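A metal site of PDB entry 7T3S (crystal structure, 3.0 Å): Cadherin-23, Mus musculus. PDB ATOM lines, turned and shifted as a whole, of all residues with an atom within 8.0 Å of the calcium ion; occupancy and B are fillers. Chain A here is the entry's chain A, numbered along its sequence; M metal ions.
The side-chain carboxylate (OD2) of Asp 38 lies close to the backbone NH (N) of Asp 5 (3.3 Å). N of Asp 94 lies within hydrogen-bond range of O of Leu 100, 2.9 Å away. N of Gly 96 is in hydrogen-bond range of OD1 of Asp 94 (3.1 Å). The side-chain amide nitrogen of Asn 4 sits at hydrogen-bond distance from the backbone carbonyl oxygen of Pro 98 (2.9 Å). O of Ile 3 lies close to ND2 of Asn 42.
O of Asn 42 binds the calcium ion (2.2 Å). O of Asn 6 binds the calcium ion (2.3 Å). The side-chain carboxylate (OD2) of Asp 36 binds the calcium ion (2.3 Å). The calcium ion is bound by OD1 of Asn 4, 2.4 Å away. OD2 of Asp 38 is bound to the calcium ion (2.4 Å). OD2 of Asp 94 is bound to the calcium ion (2.5 Å). The calcium ion has six donor atoms within binding distance. Slightly farther from the calcium ion lies the side-chain carboxylate (OD1) of Asp 36 (3.0 Å).
Within 4 Å of the calcium ion: Asn 4, Asn 6, Asp 36, Asp 38, Asn 42 and Asp 94.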
ATOM      1  N   ILE A   3      -4.949 -13.154 -22.168  1.00  0.00           N
ATOM      2  CA  ILE A   3      -6.372 -12.741 -21.947  1.00  0.00           C
ATOM      3  C   ILE A   3      -7.190 -13.924 -21.409  1.00  0.00           C
ATOM      4  O   ILE A   3      -7.130 -15.003 -21.991  1.00  0.00           O
ATOM      5  CB  ILE A   3      -7.010 -12.174 -23.242  1.00  0.00           C
ATOM      6  CG1 ILE A   3      -6.308 -10.897 -23.698  1.00  0.00           C
ATOM      7  CG2 ILE A   3      -8.521 -11.951 -23.076  1.00  0.00           C
ATOM      8  CD1 ILE A   3      -6.805 -10.350 -25.012  1.00  0.00           C
ATOM      9  N   ASN A   4      -7.939 -13.689 -20.337  1.00  0.00           N
ATOM     10  CA  ASN A   4      -8.896 -14.646 -19.744  1.00  0.00           C
ATOM     11  C   ASN A   4     -10.076 -14.748 -20.726  1.00  0.00           C
ATOM     12  O   ASN A   4     -11.040 -13.941 -20.604  1.00  0.00           O
ATOM     13  CB  ASN A   4      -9.283 -14.209 -18.322  1.00  0.00           C
ATOM     14  CG  ASN A   4      -9.824 -15.317 -17.442  1.00  0.00           C
ATOM     15  OD1 ASN A   4     -10.082 -16.424 -17.901  1.00  0.00           O
ATOM     16  ND2 ASN A   4      -9.996 -15.022 -16.166  1.00  0.00           N
ATOM     17  N   ASP A   5      -9.995 -15.713 -21.672  1.00  0.00           N
ATOM     18  CA  ASP A   5     -10.919 -15.834 -22.845  1.00  0.00           C
ATOM     19  C   ASP A   5     -12.260 -16.498 -22.481  1.00  0.00           C
ATOM     20  O   ASP A   5     -13.201 -16.341 -23.296  1.00  0.00           O
ATOM     21  CB  ASP A   5     -10.280 -16.656 -23.973  1.00  0.00           C
ATOM     22  CG  ASP A   5      -8.945 -16.139 -24.468  1.00  0.00           C
ATOM     23  OD1 ASP A   5      -8.917 -15.026 -25.058  1.00  0.00           O
ATOM     24  OD2 ASP A   5      -7.929 -16.835 -24.250  1.00  0.00           O
ATOM     25  N   ASN A   6     -12.360 -17.210 -21.334  1.00  0.00           N
ATOM     26  CA  ASN A   6     -13.541 -18.032 -20.942  1.00  0.00           C
ATOM     27  C   ASN A   6     -13.837 -17.977 -19.451  1.00  0.00           C
ATOM     28  O   ASN A   6     -12.892 -17.837 -18.667  1.00  0.00           O
ATOM     29  CB  ASN A   6     -13.338 -19.513 -21.244  1.00  0.00           C
ATOM     30  CG  ASN A   6     -13.198 -19.812 -22.710  1.00  0.00           C
ATOM     31  OD1 ASN A   6     -14.170 -19.781 -23.441  1.00  0.00           O
ATOM     32  ND2 ASN A   6     -11.980 -20.123 -23.133  1.00  0.00           N
ATOM     33  N   HIS A   7     -15.106 -18.117 -19.098  1.00  0.00           N
ATOM     34  CA  HIS A   7     -15.582 -18.422 -17.742  1.00  0.00           C
ATOM     35  C   HIS A   7     -15.451 -19.904 -17.516  1.00  0.00           C
ATOM     36  O   HIS A   7     -15.420 -20.657 -18.497  1.00  0.00           O
ATOM     37  CB  HIS A   7     -17.068 -18.089 -17.535  1.00  0.00           C
ATOM     38  CG  HIS A   7     -17.442 -16.703 -17.838  1.00  0.00           C
ATOM     39  ND1 HIS A   7     -17.316 -15.692 -16.896  1.00  0.00           N
ATOM     40  CD2 HIS A   7     -17.947 -16.146 -18.946  1.00  0.00           C
ATOM     41  CE1 HIS A   7     -17.722 -14.565 -17.430  1.00  0.00           C
ATOM     42  NE2 HIS A   7     -18.117 -14.820 -18.695  1.00  0.00           N
ATOM     43  N   PRO A   8     -15.356 -20.377 -16.253  1.00  0.00           N
ATOM     44  CA  PRO A   8     -15.581 -21.782 -15.960  1.00  0.00           C
ATOM     45  C   PRO A   8     -17.055 -22.123 -16.292  1.00  0.00           C
ATOM     46  O   PRO A   8     -17.914 -21.254 -16.140  1.00  0.00           O
ATOM     47  CB  PRO A   8     -15.280 -21.912 -14.465  1.00  0.00           C
ATOM     48  CG  PRO A   8     -14.465 -20.674 -14.144  1.00  0.00           C
ATOM     49  CD  PRO A   8     -14.995 -19.618 -15.058  1.00  0.00           C
ATOM     50  N   THR A   9     -17.289 -23.356 -16.759  1.00  0.00           N
ATOM     51  CA  THR A   9     -18.590 -23.899 -17.231  1.00  0.00           C
ATOM     52  C   THR A   9     -18.867 -25.202 -16.475  1.00  0.00           C
ATOM     53  O   THR A   9     -18.011 -26.097 -16.568  1.00  0.00           O
ATOM     54  CB  THR A   9     -18.544 -24.114 -18.765  1.00  0.00           C
ATOM     55  OG1 THR A   9     -17.963 -22.967 -19.376  1.00  0.00           O
ATOM     56  CG2 THR A   9     -19.895 -24.358 -19.397  1.00  0.00           C
ATOM     57  N   VAL A  35     -15.417 -26.893 -16.387  1.00  0.00           N
ATOM     58  CA  VAL A  35     -14.438 -26.897 -17.504  1.00  0.00           C
ATOM     59  C   VAL A  35     -14.090 -25.435 -17.912  1.00  0.00           C
ATOM     60  O   VAL A  35     -14.980 -24.559 -17.898  1.00  0.00           O
ATOM     61  CB  VAL A  35     -14.937 -27.738 -18.711  1.00  0.00           C
ATOM     62  CG1 VAL A  35     -15.303 -29.153 -18.286  1.00  0.00           C
ATOM     63  CG2 VAL A  35     -16.105 -27.113 -19.452  1.00  0.00           C
ATOM     64  N   ASP A  36     -12.822 -25.214 -18.256  1.00  0.00           N
ATOM     65  CA  ASP A  36     -12.257 -23.916 -18.706  1.00  0.00           C
ATOM     66  C   ASP A  36     -11.030 -24.226 -19.537  1.00  0.00           C
ATOM     67  O   ASP A  36      -9.986 -24.564 -18.989  1.00  0.00           O
ATOM     68  CB  ASP A  36     -11.929 -22.999 -17.526  1.00  0.00           C
ATOM     69  CG  ASP A  36     -11.554 -21.572 -17.895  1.00  0.00           C
ATOM     70  OD1 ASP A  36     -11.179 -21.344 -19.056  1.00  0.00           O
ATOM     71  OD2 ASP A  36     -11.631 -20.705 -17.017  1.00  0.00           O
ATOM     72  N   PRO A  37     -11.095 -24.115 -20.885  1.00  0.00           N
ATOM     73  CA  PRO A  37      -9.964 -24.527 -21.742  1.00  0.00           C
ATOM     74  C   PRO A  37      -8.784 -23.546 -21.767  1.00  0.00           C
ATOM     75  O   PRO A  37      -7.799 -23.850 -22.432  1.00  0.00           O
ATOM     76  CB  PRO A  37     -10.626 -24.631 -23.125  1.00  0.00           C
ATOM     77  CG  PRO A  37     -11.743 -23.602 -23.095  1.00  0.00           C
ATOM     78  CD  PRO A  37     -12.217 -23.576 -21.665  1.00  0.00           C
ATOM     79  N   ASP A  38      -8.888 -22.412 -21.064  1.00  0.00           N
ATOM     80  CA  ASP A  38      -7.817 -21.397 -20.953  1.00  0.00           C
ATOM     81  C   ASP A  38      -6.588 -22.030 -20.325  1.00  0.00           C
ATOM     82  O   ASP A  38      -6.754 -22.820 -19.403  1.00  0.00           O
ATOM     83  CB  ASP A  38      -8.283 -20.193 -20.162  1.00  0.00           C
ATOM     84  CG  ASP A  38      -9.411 -19.445 -20.820  1.00  0.00           C
ATOM     85  OD1 ASP A  38      -9.625 -19.650 -22.046  1.00  0.00           O
ATOM     86  OD2 ASP A  38     -10.078 -18.669 -20.120  1.00  0.00           O
ATOM     87  N   LEU A  39      -5.412 -21.701 -20.825  1.00  0.00           N
ATOM     88  CA  LEU A  39      -4.122 -22.187 -20.287  1.00  0.00           C
ATOM     89  C   LEU A  39      -3.685 -21.255 -19.152  1.00  0.00           C
ATOM     90  O   LEU A  39      -4.216 -20.121 -19.071  1.00  0.00           O
ATOM     91  CB  LEU A  39      -3.080 -22.244 -21.422  1.00  0.00           C
ATOM     92  CG  LEU A  39      -3.488 -23.066 -22.657  1.00  0.00           C
ATOM     93  CD1 LEU A  39      -2.317 -23.222 -23.623  1.00  0.00           C
ATOM     94  CD2 LEU A  39      -4.026 -24.448 -22.259  1.00  0.00           C
ATOM     95  N   GLY A  40      -2.767 -21.727 -18.298  1.00  0.00           N
ATOM     96  CA  GLY A  40      -2.222 -20.967 -17.167  1.00  0.00           C
ATOM     97  C   GLY A  40      -3.264 -20.740 -16.089  1.00  0.00           C
ATOM     98  O   GLY A  40      -4.177 -21.575 -15.965  1.00  0.00           O
ATOM     99  N   GLU A  41      -3.152 -19.642 -15.359  1.00  0.00           N
ATOM    100  CA  GLU A  41      -4.047 -19.299 -14.222  1.00  0.00           C
ATOM    101  C   GLU A  41      -5.434 -18.884 -14.742  1.00  0.00           C
ATOM    102  O   GLU A  41      -6.397 -18.938 -13.949  1.00  0.00           O
ATOM    103  CB  GLU A  41      -3.394 -18.239 -13.333  1.00  0.00           C
ATOM    104  CG  GLU A  41      -2.021 -18.649 -12.809  1.00  0.00           C
ATOM    105  CD  GLU A  41      -1.917 -20.090 -12.278  1.00  0.00           C
ATOM    106  OE1 GLU A  41      -2.794 -20.494 -11.455  1.00  0.00           O
ATOM    107  OE2 GLU A  41      -0.966 -20.816 -12.702  1.00  0.00           O
ATOM    108  N   ASN A  42      -5.549 -18.512 -16.036  1.00  0.00           N
ATOM    109  CA  ASN A  42      -6.839 -18.163 -16.696  1.00  0.00           C
ATOM    110  C   ASN A  42      -7.778 -19.385 -16.760  1.00  0.00           C
ATOM    111  O   ASN A  42      -8.948 -19.177 -17.039  1.00  0.00           O
ATOM    112  CB  ASN A  42      -6.615 -17.561 -18.095  1.00  0.00           C
ATOM    113  CG  ASN A  42      -6.044 -16.155 -18.070  1.00  0.00           C
ATOM    114  OD1 ASN A  42      -6.142 -15.446 -17.083  1.00  0.00           O
ATOM    115  ND2 ASN A  42      -5.438 -15.726 -19.164  1.00  0.00           N
ATOM    116  N   GLY A  43      -7.275 -20.617 -16.530  1.00  0.00           N
ATOM    117  CA  GLY A  43      -8.090 -21.857 -16.500  1.00  0.00           C
ATOM    118  C   GLY A  43      -7.862 -22.744 -15.267  1.00  0.00           C
ATOM    119  O   GLY A  43      -8.399 -23.858 -15.253  1.00  0.00           O
ATOM    120  N   THR A  44      -7.094 -22.269 -14.268  1.00  0.00           N
ATOM    121  CA  THR A  44      -6.870 -22.972 -12.966  1.00  0.00           C
ATOM    122  C   THR A  44      -8.104 -22.690 -12.094  1.00  0.00           C
ATOM    123  O   THR A  44      -8.371 -21.524 -11.856  1.00  0.00           O
ATOM    124  CB  THR A  44      -5.529 -22.528 -12.349  1.00  0.00           C
ATOM    125  OG1 THR A  44      -4.469 -22.707 -13.293  1.00  0.00           O
ATOM    126  CG2 THR A  44      -5.188 -23.271 -11.075  1.00  0.00           C
ATOM    127  N   LEU A  45      -8.831 -23.727 -11.642  1.00  0.00           N
ATOM    128  CA  LEU A  45     -10.156 -23.584 -10.944  1.00  0.00           C
ATOM    129  C   LEU A  45     -10.023 -23.685  -9.423  1.00  0.00           C
ATOM    130  O   LEU A  45      -9.158 -24.458  -8.929  1.00  0.00           O
ATOM    131  CB  LEU A  45     -11.132 -24.645 -11.458  1.00  0.00           C
ATOM    132  CG  LEU A  45     -11.404 -24.624 -12.960  1.00  0.00           C
ATOM    133  CD1 LEU A  45     -12.440 -25.646 -13.328  1.00  0.00           C
ATOM    134  CD2 LEU A  45     -11.820 -23.242 -13.426  1.00  0.00           C
ATOM    135  N   THR A  93     -14.373 -20.556  -9.520  1.00  0.00           N
ATOM    136  CA  THR A  93     -13.703 -19.376 -10.161  1.00  0.00           C
ATOM    137  C   THR A  93     -12.380 -19.841 -10.783  1.00  0.00           C
ATOM    138  O   THR A  93     -11.846 -20.864 -10.315  1.00  0.00           O
ATOM    139  CB  THR A  93     -13.540 -18.222  -9.144  1.00  0.00           C
ATOM    140  OG1 THR A  93     -13.083 -17.056  -9.819  1.00  0.00           O
ATOM    141  CG2 THR A  93     -12.575 -18.545  -8.026  1.00  0.00           C
ATOM    142  N   ASP A  94     -11.907 -19.134 -11.812  1.00  0.00           N
ATOM    143  CA  ASP A  94     -10.528 -19.277 -12.349  1.00  0.00           C
ATOM    144  C   ASP A  94      -9.666 -18.237 -11.613  1.00  0.00           C
ATOM    145  O   ASP A  94     -10.254 -17.310 -10.996  1.00  0.00           O
ATOM    146  CB  ASP A  94     -10.485 -19.174 -13.878  1.00  0.00           C
ATOM    147  CG  ASP A  94     -10.740 -17.800 -14.491  1.00  0.00           C
ATOM    148  OD1 ASP A  94     -10.354 -16.794 -13.894  1.00  0.00           O
ATOM    149  OD2 ASP A  94     -11.315 -17.757 -15.565  1.00  0.00           O
ATOM    150  N   CYS A  95      -8.340 -18.373 -11.683  1.00  0.00           N
ATOM    151  CA  CYS A  95      -7.346 -17.487 -11.003  1.00  0.00           C
ATOM    152  C   CYS A  95      -6.756 -16.468 -11.994  1.00  0.00           C
ATOM    153  O   CYS A  95      -5.682 -15.906 -11.696  1.00  0.00           O
ATOM    154  CB  CYS A  95      -6.240 -18.322 -10.376  1.00  0.00           C
ATOM    155  SG  CYS A  95      -6.861 -19.687  -9.365  1.00  0.00           S
ATOM    156  N   GLY A  96      -7.440 -16.214 -13.123  1.00  0.00           N
ATOM    157  CA  GLY A  96      -6.991 -15.304 -14.194  1.00  0.00           C
ATOM    158  C   GLY A  96      -7.043 -13.841 -13.782  1.00  0.00           C
ATOM    159  O   GLY A  96      -7.543 -13.540 -12.661  1.00  0.00           O
ATOM    160  N   ARG A  97      -6.547 -12.953 -14.658  1.00  0.00           N
ATOM    161  CA  ARG A  97      -6.572 -11.481 -14.460  1.00  0.00           C
ATOM    162  C   ARG A  97      -7.439 -10.860 -15.570  1.00  0.00           C
ATOM    163  O   ARG A  97      -7.021 -10.825 -16.719  1.00  0.00           O
ATOM    164  CB  ARG A  97      -5.139 -10.926 -14.414  1.00  0.00           C
ATOM    165  CG  ARG A  97      -4.963  -9.818 -13.371  1.00  0.00           C
ATOM    166  CD  ARG A  97      -3.514  -9.326 -13.231  1.00  0.00           C
ATOM    167  NE  ARG A  97      -3.226  -8.793 -11.885  1.00  0.00           N
ATOM    168  CZ  ARG A  97      -2.947  -9.538 -10.775  1.00  0.00           C
ATOM    169  NH1 ARG A  97      -2.710  -8.933  -9.616  1.00  0.00           N
ATOM    170  NH2 ARG A  97      -2.927 -10.873 -10.837  1.00  0.00           N
ATOM    171  N   PRO A  98      -8.690 -10.391 -15.289  1.00  0.00           N
ATOM    172  CA  PRO A  98      -9.302 -10.445 -13.967  1.00  0.00           C
ATOM    173  C   PRO A  98      -9.832 -11.839 -13.679  1.00  0.00           C
ATOM    174  O   PRO A  98     -10.059 -12.602 -14.598  1.00  0.00           O
ATOM    175  CB  PRO A  98     -10.450  -9.446 -14.082  1.00  0.00           C
ATOM    176  CG  PRO A  98     -10.875  -9.564 -15.512  1.00  0.00           C
ATOM    177  CD  PRO A  98      -9.585  -9.784 -16.274  1.00  0.00           C
ATOM    178  N   PRO A  99     -10.044 -12.197 -12.391  1.00  0.00           N
ATOM    179  CA  PRO A  99     -10.624 -13.505 -12.051  1.00  0.00           C
ATOM    180  C   PRO A  99     -12.120 -13.591 -12.401  1.00  0.00           C
ATOM    181  O   PRO A  99     -12.858 -12.671 -12.073  1.00  0.00           O
ATOM    182  CB  PRO A  99     -10.385 -13.590 -10.531  1.00  0.00           C
ATOM    183  CG  PRO A  99     -10.400 -12.153 -10.084  1.00  0.00           C
ATOM    184  CD  PRO A  99      -9.755 -11.391 -11.211  1.00  0.00           C
ATOM    185  N   LEU A 100     -12.525 -14.685 -13.073  1.00  0.00           N
ATOM    186  CA  LEU A 100     -13.915 -14.916 -13.569  1.00  0.00           C
ATOM    187  C   LEU A 100     -14.549 -16.104 -12.834  1.00  0.00           C
ATOM    188  O   LEU A 100     -13.882 -17.175 -12.726  1.00  0.00           O
ATOM    189  CB  LEU A 100     -13.878 -15.218 -15.077  1.00  0.00           C
ATOM    190  CG  LEU A 100     -13.355 -14.107 -15.970  1.00  0.00           C
ATOM    191  CD1 LEU A 100     -13.333 -14.554 -17.396  1.00  0.00           C
ATOM    192  CD2 LEU A 100     -14.179 -12.846 -15.822  1.00  0.00           C
ATOM    193  N   LYS A 101     -15.785 -15.918 -12.367  1.00  0.00           N
ATOM    194  CA  LYS A 101     -16.659 -16.991 -11.839  1.00  0.00           C
ATOM    195  C   LYS A 101     -17.463 -17.556 -12.986  1.00  0.00           C
ATOM    196  O   LYS A 101     -17.553 -16.896 -14.050  1.00  0.00           O
ATOM    197  CB  LYS A 101     -17.643 -16.462 -10.795  1.00  0.00           C
ATOM    198  CG  LYS A 101     -17.045 -15.710  -9.624  1.00  0.00           C
ATOM    199  CD  LYS A 101     -18.005 -15.604  -8.446  1.00  0.00           C
ATOM    200  CE  LYS A 101     -17.565 -14.597  -7.405  1.00  0.00           C
ATOM    201  NZ  LYS A 101     -18.525 -14.536  -6.258  1.00  0.00           N
HETATM  202 CA    CA M   1     -10.939 -18.652 -17.836  1.00  0.00          CA
